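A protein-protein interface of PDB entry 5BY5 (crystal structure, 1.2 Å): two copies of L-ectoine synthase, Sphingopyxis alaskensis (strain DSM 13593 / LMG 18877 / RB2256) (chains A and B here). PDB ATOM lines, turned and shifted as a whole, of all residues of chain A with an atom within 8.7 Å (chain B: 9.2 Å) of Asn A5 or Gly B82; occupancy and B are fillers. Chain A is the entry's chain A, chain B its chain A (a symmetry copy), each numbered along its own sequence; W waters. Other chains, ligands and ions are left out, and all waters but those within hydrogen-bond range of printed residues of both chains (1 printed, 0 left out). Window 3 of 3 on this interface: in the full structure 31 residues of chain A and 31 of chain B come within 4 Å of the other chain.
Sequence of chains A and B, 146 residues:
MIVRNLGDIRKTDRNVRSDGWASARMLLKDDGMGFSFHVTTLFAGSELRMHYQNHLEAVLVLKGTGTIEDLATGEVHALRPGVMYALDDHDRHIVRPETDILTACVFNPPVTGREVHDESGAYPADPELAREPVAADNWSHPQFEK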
ATOM      1  N   ILE A   2      -8.057  28.027 -21.512  1.00  0.00           N
ATOM      2  CA  ILE A   2      -7.876  27.217 -22.718  1.00  0.00           C
ATOM      3  C   ILE A   2      -8.074  25.759 -22.352  1.00  0.00           C
ATOM      4  O   ILE A   2      -7.568  25.306 -21.312  1.00  0.00           O
ATOM      5  CB  ILE A   2      -6.449  27.413 -23.269  1.00  0.00           C
ATOM      6  CG1 ILE A   2      -6.277  28.813 -23.853  1.00  0.00           C
ATOM      7  CG2 ILE A   2      -6.139  26.343 -24.275  1.00  0.00           C
ATOM      8  CD1 ILE A   2      -4.831  29.141 -24.165  1.00  0.00           C
ATOM      9  N   VAL A   3      -8.802  25.024 -23.192  1.00  0.00           N
ATOM     10  CA  VAL A   3      -8.886  23.570 -23.083  1.00  0.00           C
ATOM     11  C   VAL A   3      -8.783  22.983 -24.449  1.00  0.00           C
ATOM     12  O   VAL A   3      -9.584  23.341 -25.326  1.00  0.00           O
ATOM     13  CB  VAL A   3     -10.172  23.071 -22.398  1.00  0.00           C
ATOM     14  CG1 VAL A   3     -10.053  21.550 -22.220  1.00  0.00           C
ATOM     15  CG2 VAL A   3     -10.467  23.772 -21.106  1.00  0.00           C
ATOM     16  N   ARG A   4      -7.792  22.138 -24.725  1.00  0.00           N
ATOM     17  CA  ARG A   4      -7.520  21.602 -26.065  1.00  0.00           C
ATOM     18  C   ARG A   4      -7.076  20.177 -25.941  1.00  0.00           C
ATOM     19  O   ARG A   4      -6.583  19.750 -24.923  1.00  0.00           O
ATOM     20  CB  ARG A   4      -6.371  22.324 -26.736  1.00  0.00           C
ATOM     21  CG  ARG A   4      -6.597  23.703 -26.918  1.00  0.00           C
ATOM     22  CD  ARG A   4      -5.335  24.373 -27.480  1.00  0.00           C
ATOM     23  NE  ARG A   4      -5.852  25.666 -27.631  1.00  0.00           N
ATOM     24  CZ  ARG A   4      -5.165  26.774 -27.725  1.00  0.00           C
ATOM     25  NH1 ARG A   4      -3.831  26.787 -27.693  1.00  0.00           N
ATOM     26  NH2 ARG A   4      -5.850  27.900 -27.826  1.00  0.00           N
ATOM     27  N   ASN A   5      -7.304  19.450 -27.009  1.00  0.00           N
ATOM     28  CA  ASN A   5      -7.058  18.002 -27.098  1.00  0.00           C
ATOM     29  C   ASN A   5      -5.848  17.768 -28.058  1.00  0.00           C
ATOM     30  O   ASN A   5      -5.771  18.355 -29.163  1.00  0.00           O
ATOM     31  CB  ASN A   5      -8.359  17.206 -27.652  1.00  0.00           C
ATOM     32  CG  ASN A   5      -9.696  17.555 -26.952  1.00  0.00           C
ATOM     33  OD1 ASN A   5     -10.647  17.651 -27.650  1.00  0.00           O
ATOM     34  ND2 ASN A   5      -9.766  17.773 -25.581  1.00  0.00           N
ATOM     35  N   LEU A   6      -4.960  16.839 -27.686  1.00  0.00           N
ATOM     36  CA  LEU A   6      -3.873  16.417 -28.552  1.00  0.00           C
ATOM     37  C   LEU A   6      -4.354  15.884 -29.890  1.00  0.00           C
ATOM     38  O   LEU A   6      -3.794  16.202 -30.937  1.00  0.00           O
ATOM     39  CB  LEU A   6      -3.071  15.353 -27.817  1.00  0.00           C
ATOM     40  CG  LEU A   6      -1.930  14.717 -28.558  1.00  0.00           C
ATOM     41  CD1 LEU A   6      -0.897  15.745 -28.998  1.00  0.00           C
ATOM     42  CD2 LEU A   6      -1.315  13.707 -27.612  1.00  0.00           C
ATOM     43  N   GLY A   7      -5.407  15.089 -29.880  1.00  0.00           N
ATOM     44  CA  GLY A   7      -5.886  14.529 -31.119  1.00  0.00           C
ATOM     45  C   GLY A   7      -6.360  15.572 -32.098  1.00  0.00           C
ATOM     46  O   GLY A   7      -6.134  15.408 -33.307  1.00  0.00           O
ATOM     47  N   ASP A   8      -6.980  16.636 -31.614  1.00  0.00           N
ATOM     48  CA  ASP A   8      -7.370  17.734 -32.481  1.00  0.00           C
ATOM     49  C   ASP A   8      -6.162  18.471 -33.023  1.00  0.00           C
ATOM     50  O   ASP A   8      -6.097  18.755 -34.209  1.00  0.00           O
ATOM     51  CB  ASP A   8      -8.264  18.742 -31.751  1.00  0.00           C
ATOM     52  CG  ASP A   8      -9.619  18.238 -31.440  1.00  0.00           C
ATOM     53  OD1 ASP A   8     -10.069  17.248 -32.012  1.00  0.00           O
ATOM     54  OD2 ASP A   8     -10.262  18.906 -30.578  1.00  0.00           O
ATOM     55  N   ILE A   9      -5.209  18.812 -32.166  1.00  0.00           N
ATOM     56  CA  ILE A   9      -4.037  19.552 -32.598  1.00  0.00           C
ATOM     57  C   ILE A   9      -3.226  18.783 -33.626  1.00  0.00           C
ATOM     58  O   ILE A   9      -2.658  19.383 -34.543  1.00  0.00           O
ATOM     59  CB  ILE A   9      -3.225  20.018 -31.361  1.00  0.00           C
ATOM     60  CG1 ILE A   9      -4.075  20.949 -30.466  1.00  0.00           C
ATOM     61  CG2 ILE A   9      -1.923  20.646 -31.757  1.00  0.00           C
ATOM     62  CD1 ILE A   9      -4.608  22.221 -31.107  1.00  0.00           C
ATOM     63  N   ARG A  10      -3.178  17.462 -33.452  1.00  0.00           N
ATOM     64  CA  ARG A  10      -2.422  16.611 -34.366  1.00  0.00           C
ATOM     65  C   ARG A  10      -2.918  16.669 -35.792  1.00  0.00           C
ATOM     66  O   ARG A  10      -2.178  16.311 -36.695  1.00  0.00           O
ATOM     67  CB  ARG A  10      -2.407  15.144 -33.899  1.00  0.00           C
ATOM     68  CG  ARG A  10      -1.397  14.934 -32.823  1.00  0.00           C
ATOM     69  CD  ARG A  10      -0.824  13.562 -32.814  1.00  0.00           C
ATOM     70  NE  ARG A  10       0.323  13.511 -31.934  1.00  0.00           N
ATOM     71  CZ  ARG A  10       1.647  13.934 -32.117  1.00  0.00           C
ATOM     72  NH1 ARG A  10       2.327  14.446 -33.211  1.00  0.00           N
ATOM     73  NH2 ARG A  10       2.429  13.784 -31.065  1.00  0.00           N
ATOM     74  N   LYS A  11      -4.164  17.082 -35.989  1.00  0.00           N
ATOM     75  CA  LYS A  11      -4.748  17.165 -37.297  1.00  0.00           C
ATOM     76  C   LYS A  11      -4.570  18.534 -37.933  1.00  0.00           C
ATOM     77  O   LYS A  11      -5.221  18.768 -38.968  1.00  0.00           O
ATOM     78  CB  LYS A  11      -6.237  16.827 -37.204  1.00  0.00           C
ATOM     79  CG  LYS A  11      -6.517  15.425 -36.703  1.00  0.00           C
ATOM     80  CD  LYS A  11      -7.984  15.083 -36.836  1.00  0.00           C
ATOM     81  CE  LYS A  11      -8.873  15.811 -35.832  1.00  0.00           C
ATOM     82  NZ  LYS A  11     -10.295  15.333 -35.884  1.00  0.00           N
ATOM     83  N   THR A  12      -3.690  19.396 -37.394  1.00  0.00           N
ATOM     84  CA  THR A  12      -3.522  20.774 -37.816  1.00  0.00           C
ATOM     85  C   THR A  12      -2.068  21.101 -38.114  1.00  0.00           C
ATOM     86  O   THR A  12      -1.174  20.303 -37.824  1.00  0.00           O
ATOM     87  CB  THR A  12      -4.048  21.758 -36.758  1.00  0.00           C
ATOM     88  OG1 THR A  12      -3.133  21.850 -35.655  1.00  0.00           O
ATOM     89  CG2 THR A  12      -5.428  21.379 -36.230  1.00  0.00           C
ATOM     90  N   ALA A  24       3.301  18.044 -31.648  1.00  0.00           N
ATOM     91  CA  ALA A  24       2.045  18.747 -31.569  1.00  0.00           C
ATOM     92  C   ALA A  24       2.214  19.918 -30.588  1.00  0.00           C
ATOM     93  O   ALA A  24       2.413  19.733 -29.401  1.00  0.00           O
ATOM     94  CB  ALA A  24       0.947  17.835 -31.074  1.00  0.00           C
ATOM     95  N   ARG A  25       2.128  21.128 -31.120  1.00  0.00           N
ATOM     96  CA  ARG A  25       2.346  22.354 -30.353  1.00  0.00           C
ATOM     97  C   ARG A  25       0.966  22.747 -29.776  1.00  0.00           C
ATOM     98  O   ARG A  25       0.082  23.278 -30.436  1.00  0.00           O
ATOM     99  CB  ARG A  25       3.038  23.433 -31.235  1.00  0.00           C
ATOM    100  CG  ARG A  25       4.553  23.201 -31.582  1.00  0.00           C
ATOM    101  CD  ARG A  25       5.072  23.511 -33.129  1.00  0.00           C
ATOM    102  NE  ARG A  25       6.594  23.545 -33.415  1.00  0.00           N
ATOM    103  CZ  ARG A  25       7.407  22.696 -32.725  1.00  0.00           C
ATOM    104  NH1 ARG A  25       6.837  21.842 -32.016  1.00  0.00           N
ATOM    105  NH2 ARG A  25       8.751  22.637 -32.693  1.00  0.00           N
ATOM    106  N   MET A  26       0.820  22.431 -28.490  1.00  0.00           N
ATOM    107  CA  MET A  26      -0.373  22.750 -27.719  1.00  0.00           C
ATOM    108  C   MET A  26      -0.477  24.248 -27.406  1.00  0.00           C
ATOM    109  O   MET A  26      -1.512  24.878 -27.625  1.00  0.00           O
ATOM    110  CB  MET A  26      -0.371  21.918 -26.426  1.00  0.00           C
ATOM    111  CG  MET A  26      -0.369  20.403 -26.660  1.00  0.00           C
ATOM    112  SD  MET A  26      -1.642  19.746 -27.810  1.00  0.00           S
ATOM    113  CE  MET A  26      -3.015  19.763 -26.678  1.00  0.00           C
ATOM    114  N   VAL A  39       3.757  18.227 -27.308  1.00  0.00           N
ATOM    115  CA  VAL A  39       3.767  16.776 -27.130  1.00  0.00           C
ATOM    116  C   VAL A  39       4.561  16.253 -28.330  1.00  0.00           C
ATOM    117  O   VAL A  39       4.110  16.340 -29.468  1.00  0.00           O
ATOM    118  CB  VAL A  39       2.382  16.164 -27.055  1.00  0.00           C
ATOM    119  CG1 VAL A  39       2.506  14.666 -26.968  1.00  0.00           C
ATOM    120  CG2 VAL A  39       1.635  16.719 -25.853  1.00  0.00           C
ATOM    121  N   LEU A  62       7.165  10.379 -21.392  1.00  0.00           N
ATOM    122  CA  LEU A  62       5.863   9.799 -21.087  1.00  0.00           C
ATOM    123  C   LEU A  62       5.809   8.326 -21.422  1.00  0.00           C
ATOM    124  O   LEU A  62       5.166   7.561 -20.705  1.00  0.00           O
ATOM    125  CB  LEU A  62       4.760  10.543 -21.836  1.00  0.00           C
ATOM    126  CG  LEU A  62       4.733  12.057 -21.659  1.00  0.00           C
ATOM    127  CD1 LEU A  62       3.589  12.645 -22.440  1.00  0.00           C
ATOM    128  CD2 LEU A  62       4.662  12.466 -20.207  1.00  0.00           C
ATOM    129  N   LYS A  63       6.383   7.944 -22.552  1.00  0.00           N
ATOM    130  CA  LYS A  63       6.353   6.565 -23.049  1.00  0.00           C
ATOM    131  C   LYS A  63       7.695   6.317 -23.747  1.00  0.00           C
ATOM    132  O   LYS A  63       8.285   7.250 -24.307  1.00  0.00           O
ATOM    133  CB  LYS A  63       5.236   6.373 -24.068  1.00  0.00           C
ATOM    134  CG  LYS A  63       3.828   6.677 -23.556  1.00  0.00           C
ATOM    135  CD  LYS A  63       2.724   6.341 -24.552  1.00  0.00           C
ATOM    136  CE  LYS A  63       1.332   6.741 -24.002  1.00  0.00           C
ATOM    137  NZ  LYS A  63       0.250   6.534 -24.991  1.00  0.00           N
ATOM    138  N   LEU A 102       7.600   9.209 -26.468  1.00  0.00           N
ATOM    139  CA  LEU A 102       6.639  10.293 -26.371  1.00  0.00           C
ATOM    140  C   LEU A 102       7.033  11.182 -25.206  1.00  0.00           C
ATOM    141  O   LEU A 102       7.331  10.671 -24.116  1.00  0.00           O
ATOM    142  CB  LEU A 102       5.237   9.718 -26.119  1.00  0.00           C
ATOM    143  CG  LEU A 102       4.106  10.729 -26.153  1.00  0.00           C
ATOM    144  CD1 LEU A 102       3.873  11.278 -27.552  1.00  0.00           C
ATOM    145  CD2 LEU A 102       2.850  10.108 -25.596  1.00  0.00           C
ATOM    146  N   VAL B  59      -1.663  22.479 -17.827  1.00  0.00           N
ATOM    147  CA  VAL B  59      -1.827  21.124 -17.314  1.00  0.00           C
ATOM    148  C   VAL B  59      -2.129  20.166 -18.435  1.00  0.00           C
ATOM    149  O   VAL B  59      -3.095  20.375 -19.163  1.00  0.00           O
ATOM    150  CB  VAL B  59      -2.976  21.071 -16.290  1.00  0.00           C
ATOM    151  CG1 VAL B  59      -3.130  19.659 -15.756  1.00  0.00           C
ATOM    152  CG2 VAL B  59      -2.723  22.065 -15.171  1.00  0.00           C
ATOM    153  N   LEU B  60      -1.291  19.143 -18.608  1.00  0.00           N
ATOM    154  CA  LEU B  60      -1.526  18.090 -19.561  1.00  0.00           C
ATOM    155  C   LEU B  60      -1.943  16.827 -18.820  1.00  0.00           C
ATOM    156  O   LEU B  60      -1.212  16.346 -17.979  1.00  0.00           O
ATOM    157  CB  LEU B  60      -0.280  17.798 -20.394  1.00  0.00           C
ATOM    158  CG  LEU B  60      -0.379  16.692 -21.416  1.00  0.00           C
ATOM    159  CD1 LEU B  60      -1.349  17.005 -22.513  1.00  0.00           C
ATOM    160  CD2 LEU B  60       0.983  16.372 -21.984  1.00  0.00           C
ATOM    161  N   VAL B  61      -3.105  16.267 -19.174  1.00  0.00           N
ATOM    162  CA  VAL B  61      -3.560  15.025 -18.596  1.00  0.00           C
ATOM    163  C   VAL B  61      -2.830  13.855 -19.204  1.00  0.00           C
ATOM    164  O   VAL B  61      -2.827  13.680 -20.426  1.00  0.00           O
ATOM    165  CB  VAL B  61      -5.059  14.871 -18.746  1.00  0.00           C
ATOM    166  CG1 VAL B  61      -5.523  13.536 -18.155  1.00  0.00           C
ATOM    167  CG2 VAL B  61      -5.821  16.011 -18.068  1.00  0.00           C
ATOM    168  N   LEU B  62      -2.208  13.044 -18.346  1.00  0.00           N
ATOM    169  CA  LEU B  62      -1.438  11.879 -18.764  1.00  0.00           C
ATOM    170  C   LEU B  62      -2.226  10.597 -18.608  1.00  0.00           C
ATOM    171  O   LEU B  62      -2.092   9.696 -19.433  1.00  0.00           O
ATOM    172  CB  LEU B  62      -0.135  11.788 -17.973  1.00  0.00           C
ATOM    173  CG  LEU B  62       0.736  13.039 -17.970  1.00  0.00           C
ATOM    174  CD1 LEU B  62       1.985  12.793 -17.167  1.00  0.00           C
ATOM    175  CD2 LEU B  62       1.074  13.507 -19.365  1.00  0.00           C
ATOM    176  N   LYS B  63      -2.955  10.468 -17.510  1.00  0.00           N
ATOM    177  CA  LYS B  63      -3.715   9.260 -17.182  1.00  0.00           C
ATOM    178  C   LYS B  63      -4.993   9.721 -16.470  1.00  0.00           C
ATOM    179  O   LYS B  63      -4.984  10.749 -15.782  1.00  0.00           O
ATOM    180  CB  LYS B  63      -2.932   8.360 -16.233  1.00  0.00           C
ATOM    181  CG  LYS B  63      -1.576   7.886 -16.756  1.00  0.00           C
ATOM    182  CD  LYS B  63      -0.883   6.879 -15.847  1.00  0.00           C
ATOM    183  CE  LYS B  63       0.515   6.497 -16.396  1.00  0.00           C
ATOM    184  NZ  LYS B  63       1.262   5.608 -15.479  1.00  0.00           N
ATOM    185  N   GLY B  64      -6.061   8.944 -16.632  1.00  0.00           N
ATOM    186  CA  GLY B  64      -7.280   9.118 -15.870  1.00  0.00           C
ATOM    187  C   GLY B  64      -8.316   9.991 -16.536  1.00  0.00           C
ATOM    188  O   GLY B  64      -8.073  10.626 -17.551  1.00  0.00           O
ATOM    189  N   ILE B  68     -13.255  19.276 -16.018  1.00  0.00           N
ATOM    190  CA  ILE B  68     -12.949  20.631 -15.564  1.00  0.00           C
ATOM    191  C   ILE B  68     -14.106  21.529 -16.007  1.00  0.00           C
ATOM    192  O   ILE B  68     -14.462  21.558 -17.190  1.00  0.00           O
ATOM    193  CB  ILE B  68     -11.573  21.188 -16.034  1.00  0.00           C
ATOM    194  CG1 ILE B  68     -11.341  22.586 -15.452  1.00  0.00           C
ATOM    195  CG2 ILE B  68     -11.393  21.180 -17.541  1.00  0.00           C
ATOM    196  CD1 ILE B  68      -9.935  23.112 -15.666  1.00  0.00           C
ATOM    197  N   HIS B  77     -15.791  20.466 -19.424  1.00  0.00           N
ATOM    198  CA  HIS B  77     -14.866  19.850 -20.356  1.00  0.00           C
ATOM    199  C   HIS B  77     -14.432  18.479 -19.828  1.00  0.00           C
ATOM    200  O   HIS B  77     -14.126  18.315 -18.666  1.00  0.00           O
ATOM    201  CB  HIS B  77     -13.594  20.692 -20.481  1.00  0.00           C
ATOM    202  CG  HIS B  77     -13.802  22.101 -20.884  1.00  0.00           C
ATOM    203  ND1 HIS B  77     -13.754  22.516 -22.183  1.00  0.00           N
ATOM    204  CD2 HIS B  77     -14.040  23.222 -20.154  1.00  0.00           C
ATOM    205  CE1 HIS B  77     -13.926  23.823 -22.265  1.00  0.00           C
ATOM    206  NE2 HIS B  77     -14.097  24.287 -21.042  1.00  0.00           N
ATOM    207  N   ALA B  78     -14.342  17.510 -20.729  1.00  0.00           N
ATOM    208  CA  ALA B  78     -13.826  16.209 -20.402  1.00  0.00           C
ATOM    209  C   ALA B  78     -12.319  16.280 -20.169  1.00  0.00           C
ATOM    210  O   ALA B  78     -11.587  16.890 -20.931  1.00  0.00           O
ATOM    211  CB  ALA B  78     -14.085  15.243 -21.535  1.00  0.00           C
ATOM    212  N   LEU B  79     -11.859  15.644 -19.085  1.00  0.00           N
ATOM    213  CA  LEU B  79     -10.447  15.359 -18.882  1.00  0.00           C
ATOM    214  C   LEU B  79     -10.208  13.902 -19.187  1.00  0.00           C
ATOM    215  O   LEU B  79     -10.900  13.018 -18.654  1.00  0.00           O
ATOM    216  CB  LEU B  79     -10.020  15.699 -17.463  1.00  0.00           C
ATOM    217  CG  LEU B  79     -10.171  17.144 -17.039  1.00  0.00           C
ATOM    218  CD1 LEU B  79      -9.743  17.348 -15.606  1.00  0.00           C
ATOM    219  CD2 LEU B  79      -9.416  18.066 -17.960  1.00  0.00           C
ATOM    220  N   ARG B  80      -9.216  13.638 -20.011  1.00  0.00           N
ATOM    221  CA  ARG B  80      -8.762  12.285 -20.379  1.00  0.00           C
ATOM    222  C   ARG B  80      -7.352  12.472 -20.922  1.00  0.00           C
ATOM    223  O   ARG B  80      -6.941  13.612 -21.198  1.00  0.00           O
ATOM    224  CB  ARG B  80      -9.714  11.634 -21.327  1.00  0.00           C
ATOM    225  CG  ARG B  80      -9.959  12.386 -22.585  1.00  0.00           C
ATOM    226  CD  ARG B  80     -10.999  11.619 -23.505  1.00  0.00           C
ATOM    227  NE  ARG B  80     -12.417  11.532 -23.049  1.00  0.00           N
ATOM    228  CZ  ARG B  80     -13.461  12.290 -23.480  1.00  0.00           C
ATOM    229  NH1 ARG B  80     -13.254  13.268 -24.378  1.00  0.00           N
ATOM    230  NH2 ARG B  80     -14.736  12.081 -23.027  1.00  0.00           N
ATOM    231  N   PRO B  81      -6.616  11.398 -21.117  1.00  0.00           N
ATOM    232  CA  PRO B  81      -5.245  11.554 -21.604  1.00  0.00           C
ATOM    233  C   PRO B  81      -5.214  12.328 -22.903  1.00  0.00           C
ATOM    234  O   PRO B  81      -5.971  12.083 -23.832  1.00  0.00           O
ATOM    235  CB  PRO B  81      -4.783  10.088 -21.808  1.00  0.00           C
ATOM    236  CG  PRO B  81      -5.547   9.364 -20.714  1.00  0.00           C
ATOM    237  CD  PRO B  81      -6.920  10.009 -20.747  1.00  0.00           C
ATOM    238  N   GLY B  82      -4.321  13.313 -22.938  1.00  0.00           N
ATOM    239  CA  GLY B  82      -4.134  14.182 -24.065  1.00  0.00           C
ATOM    240  C   GLY B  82      -4.860  15.514 -24.011  1.00  0.00           C
ATOM    241  O   GLY B  82      -4.617  16.374 -24.867  1.00  0.00           O
ATOM    242  N   VAL B  83      -5.707  15.721 -23.006  1.00  0.00           N
ATOM    243  CA  VAL B  83      -6.341  17.016 -22.823  1.00  0.00           C
ATOM    244  C   VAL B  83      -5.386  17.912 -22.057  1.00  0.00           C
ATOM    245  O   VAL B  83      -4.773  17.524 -21.065  1.00  0.00           O
ATOM    246  CB  VAL B  83      -7.647  16.874 -22.039  1.00  0.00           C
ATOM    247  CG1 VAL B  83      -8.268  18.225 -21.747  1.00  0.00           C
ATOM    248  CG2 VAL B  83      -8.642  16.056 -22.822  1.00  0.00           C
ATOM    249  N   MET B  84      -5.271  19.143 -22.521  1.00  0.00           N
ATOM    250  CA  MET B  84      -4.470  20.174 -21.891  1.00  0.00           C
ATOM    251  C   MET B  84      -5.377  21.355 -21.535  1.00  0.00           C
ATOM    252  O   MET B  84      -6.146  21.806 -22.390  1.00  0.00           O
ATOM    253  CB  MET B  84      -3.367  20.643 -22.816  1.00  0.00           C
ATOM    254  CG  MET B  84      -2.341  21.587 -22.198  1.00  0.00           C
ATOM    255  SD  MET B  84      -1.602  22.771 -23.169  1.00  0.00           S
ATOM    256  CE  MET B  84      -3.072  23.603 -22.808  1.00  0.00           C
ATOM    257  N   TYR B  85      -5.252  21.876 -20.322  1.00  0.00           N
ATOM    258  CA  TYR B  85      -5.928  23.123 -20.005  1.00  0.00           C
ATOM    259  C   TYR B  85      -4.909  24.126 -19.514  1.00  0.00           C
ATOM    260  O   TYR B  85      -3.847  23.788 -19.008  1.00  0.00           O
ATOM    261  CB  TYR B  85      -7.092  22.897 -19.039  1.00  0.00           C
ATOM    262  CG  TYR B  85      -6.803  22.282 -17.696  1.00  0.00           C
ATOM    263  CD1 TYR B  85      -6.436  23.067 -16.613  1.00  0.00           C
ATOM    264  CD2 TYR B  85      -6.886  20.919 -17.486  1.00  0.00           C
ATOM    265  CE1 TYR B  85      -6.204  22.516 -15.374  1.00  0.00           C
ATOM    266  CE2 TYR B  85      -6.669  20.376 -16.222  1.00  0.00           C
ATOM    267  CZ  TYR B  85      -6.316  21.193 -15.153  1.00  0.00           C
ATOM    268  OH  TYR B  85      -6.063  20.628 -13.929  1.00  0.00           O
ATOM    269  N   ILE B 101      -6.226  11.235 -11.482  1.00  0.00           N
ATOM    270  CA  ILE B 101      -5.705  11.815 -12.727  1.00  0.00           C
ATOM    271  C   ILE B 101      -4.230  12.144 -12.523  1.00  0.00           C
ATOM    272  O   ILE B 101      -3.889  12.800 -11.535  1.00  0.00           O
ATOM    273  CB  ILE B 101      -6.493  13.068 -13.127  1.00  0.00           C
ATOM    274  CG1 ILE B 101      -7.933  12.705 -13.492  1.00  0.00           C
ATOM    275  CG2 ILE B 101      -5.839  13.735 -14.311  1.00  0.00           C
ATOM    276  CD1 ILE B 101      -8.805  13.893 -13.807  1.00  0.00           C
ATOM    277  N   LEU B 102      -3.403  11.724 -13.432  1.00  0.00           N
ATOM    278  CA  LEU B 102      -1.998  12.091 -13.434  1.00  0.00           C
ATOM    279  C   LEU B 102      -1.788  13.180 -14.471  1.00  0.00           C
ATOM    280  O   LEU B 102      -2.281  13.054 -15.602  1.00  0.00           O
ATOM    281  CB  LEU B 102      -1.146  10.868 -13.803  1.00  0.00           C
ATOM    282  CG  LEU B 102       0.355  11.067 -13.691  1.00  0.00           C
ATOM    283  CD1 LEU B 102       0.803  11.223 -12.245  1.00  0.00           C
ATOM    284  CD2 LEU B 102       1.072   9.923 -14.362  1.00  0.00           C
ATOM    285  N   THR B 103      -1.069  14.223 -14.088  1.00  0.00           N
ATOM    286  CA  THR B 103      -0.854  15.367 -14.946  1.00  0.00           C
ATOM    287  C   THR B 103       0.610  15.811 -14.947  1.00  0.00           C
ATOM    288  O   THR B 103       1.342  15.559 -13.998  1.00  0.00           O
ATOM    289  CB  THR B 103      -1.704  16.580 -14.484  1.00  0.00           C
ATOM    290  OG1 THR B 103      -1.279  17.055 -13.230  1.00  0.00           O
ATOM    291  CG2 THR B 103      -3.192  16.272 -14.431  1.00  0.00           C
HETATM  292  O   HOH W   1     -11.797  17.985 -23.477  1.00  0.00           O
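The backbone NH (N) of Met B84 lies within hydrogen-bond range of the backbone carbonyl oxygen (O) of Arg A4 (2.8 Å). N of Leu A6 is in hydrogen-bond range of O of Gly B82, at 2.9 Å.
The backbone carbonyl oxygen of Ile B68 is in hydrogen-bond range of the backbone NH of His B77. O of Val A39 sits at hydrogen-bond distance from N of Ala A24. The backbone NH of Gly B82 lies within hydrogen-bond range of the backbone carbonyl oxygen of Val B61. The backbone carbonyl oxygen of Val B83 is in hydrogen-bond range of the backbone NH of Val B61 (2.8 Å). The backbone carbonyl oxygen of Val A39 is in hydrogen-bond range of the guanidinium group of Arg A10 (3.5 Å). The backbone carbonyl oxygen (O) of Tyr B85 is in hydrogen-bond range of the backbone NH (N) of Val B59, at 2.8 Å.
Ile A2 touches Met B84. His B77 touches Val A3. Val B83 touches Val A3 (CG1 to CG1, 3.8 Å). Met B84 touches Val A3. O of Gly B82 touches O of Arg A4 (3.9 Å). Asn A5 touches Gly B82 (CA to O, 3.7 Å). Val B83 touches Asn A5. Met A26 touches Met B84. Val A39 touches Leu B60. Leu A62 touches Leu B62.
Of the printed residues of chain B, Ile A2 touches Met B84 and Tyr B85. Printed residues of chain B within 4 Å of Asn A5: Gly B82 and Val B83. Of the printed residues of chain B, Leu A6 touches Gly B82. No residue of chain B comes within 4 Å of Gly A7. No residue of chain B comes within 4 Å of Asp A8. Of the printed residues of chain B, Met A26 touches Met B84 (3.6 Å). Of the printed residues of chain A, Leu B60 touches Val A39 (3.9 Å). Lys B63 touches none of the printed residues of chain A. Printed residues of chain A within 4 Å of Gly B82: Arg A4, Asn A5 and Leu A6. Leu B102 touches none of the printed residues of chain A.
Of the 19 printed residues of chain B, 7 touch a printed residue of chain A. Hydrophobic or aromatic side chains of chain B within 4 Å of the printed part of chain A: Leu B60, Leu B62, His B77, Val B83, Met B84 and Tyr B85. Among the printed residues, no Asp or Glu carboxylate lies within 4 Å of a Lys or Arg side-chain nitrogen of the other chain.
Leu B62 touches its own counterpart, Leu A62. Of the 14 pairs that touch across the chains among the printed residues, 1 has its exchanged pair printed and touching as well.
Water W1 bridges the backbone carbonyl oxygen (O) of Ala B78 (2.8 Å) and the side-chain amide nitrogen (ND2) of Asn A5 (2.9 Å).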
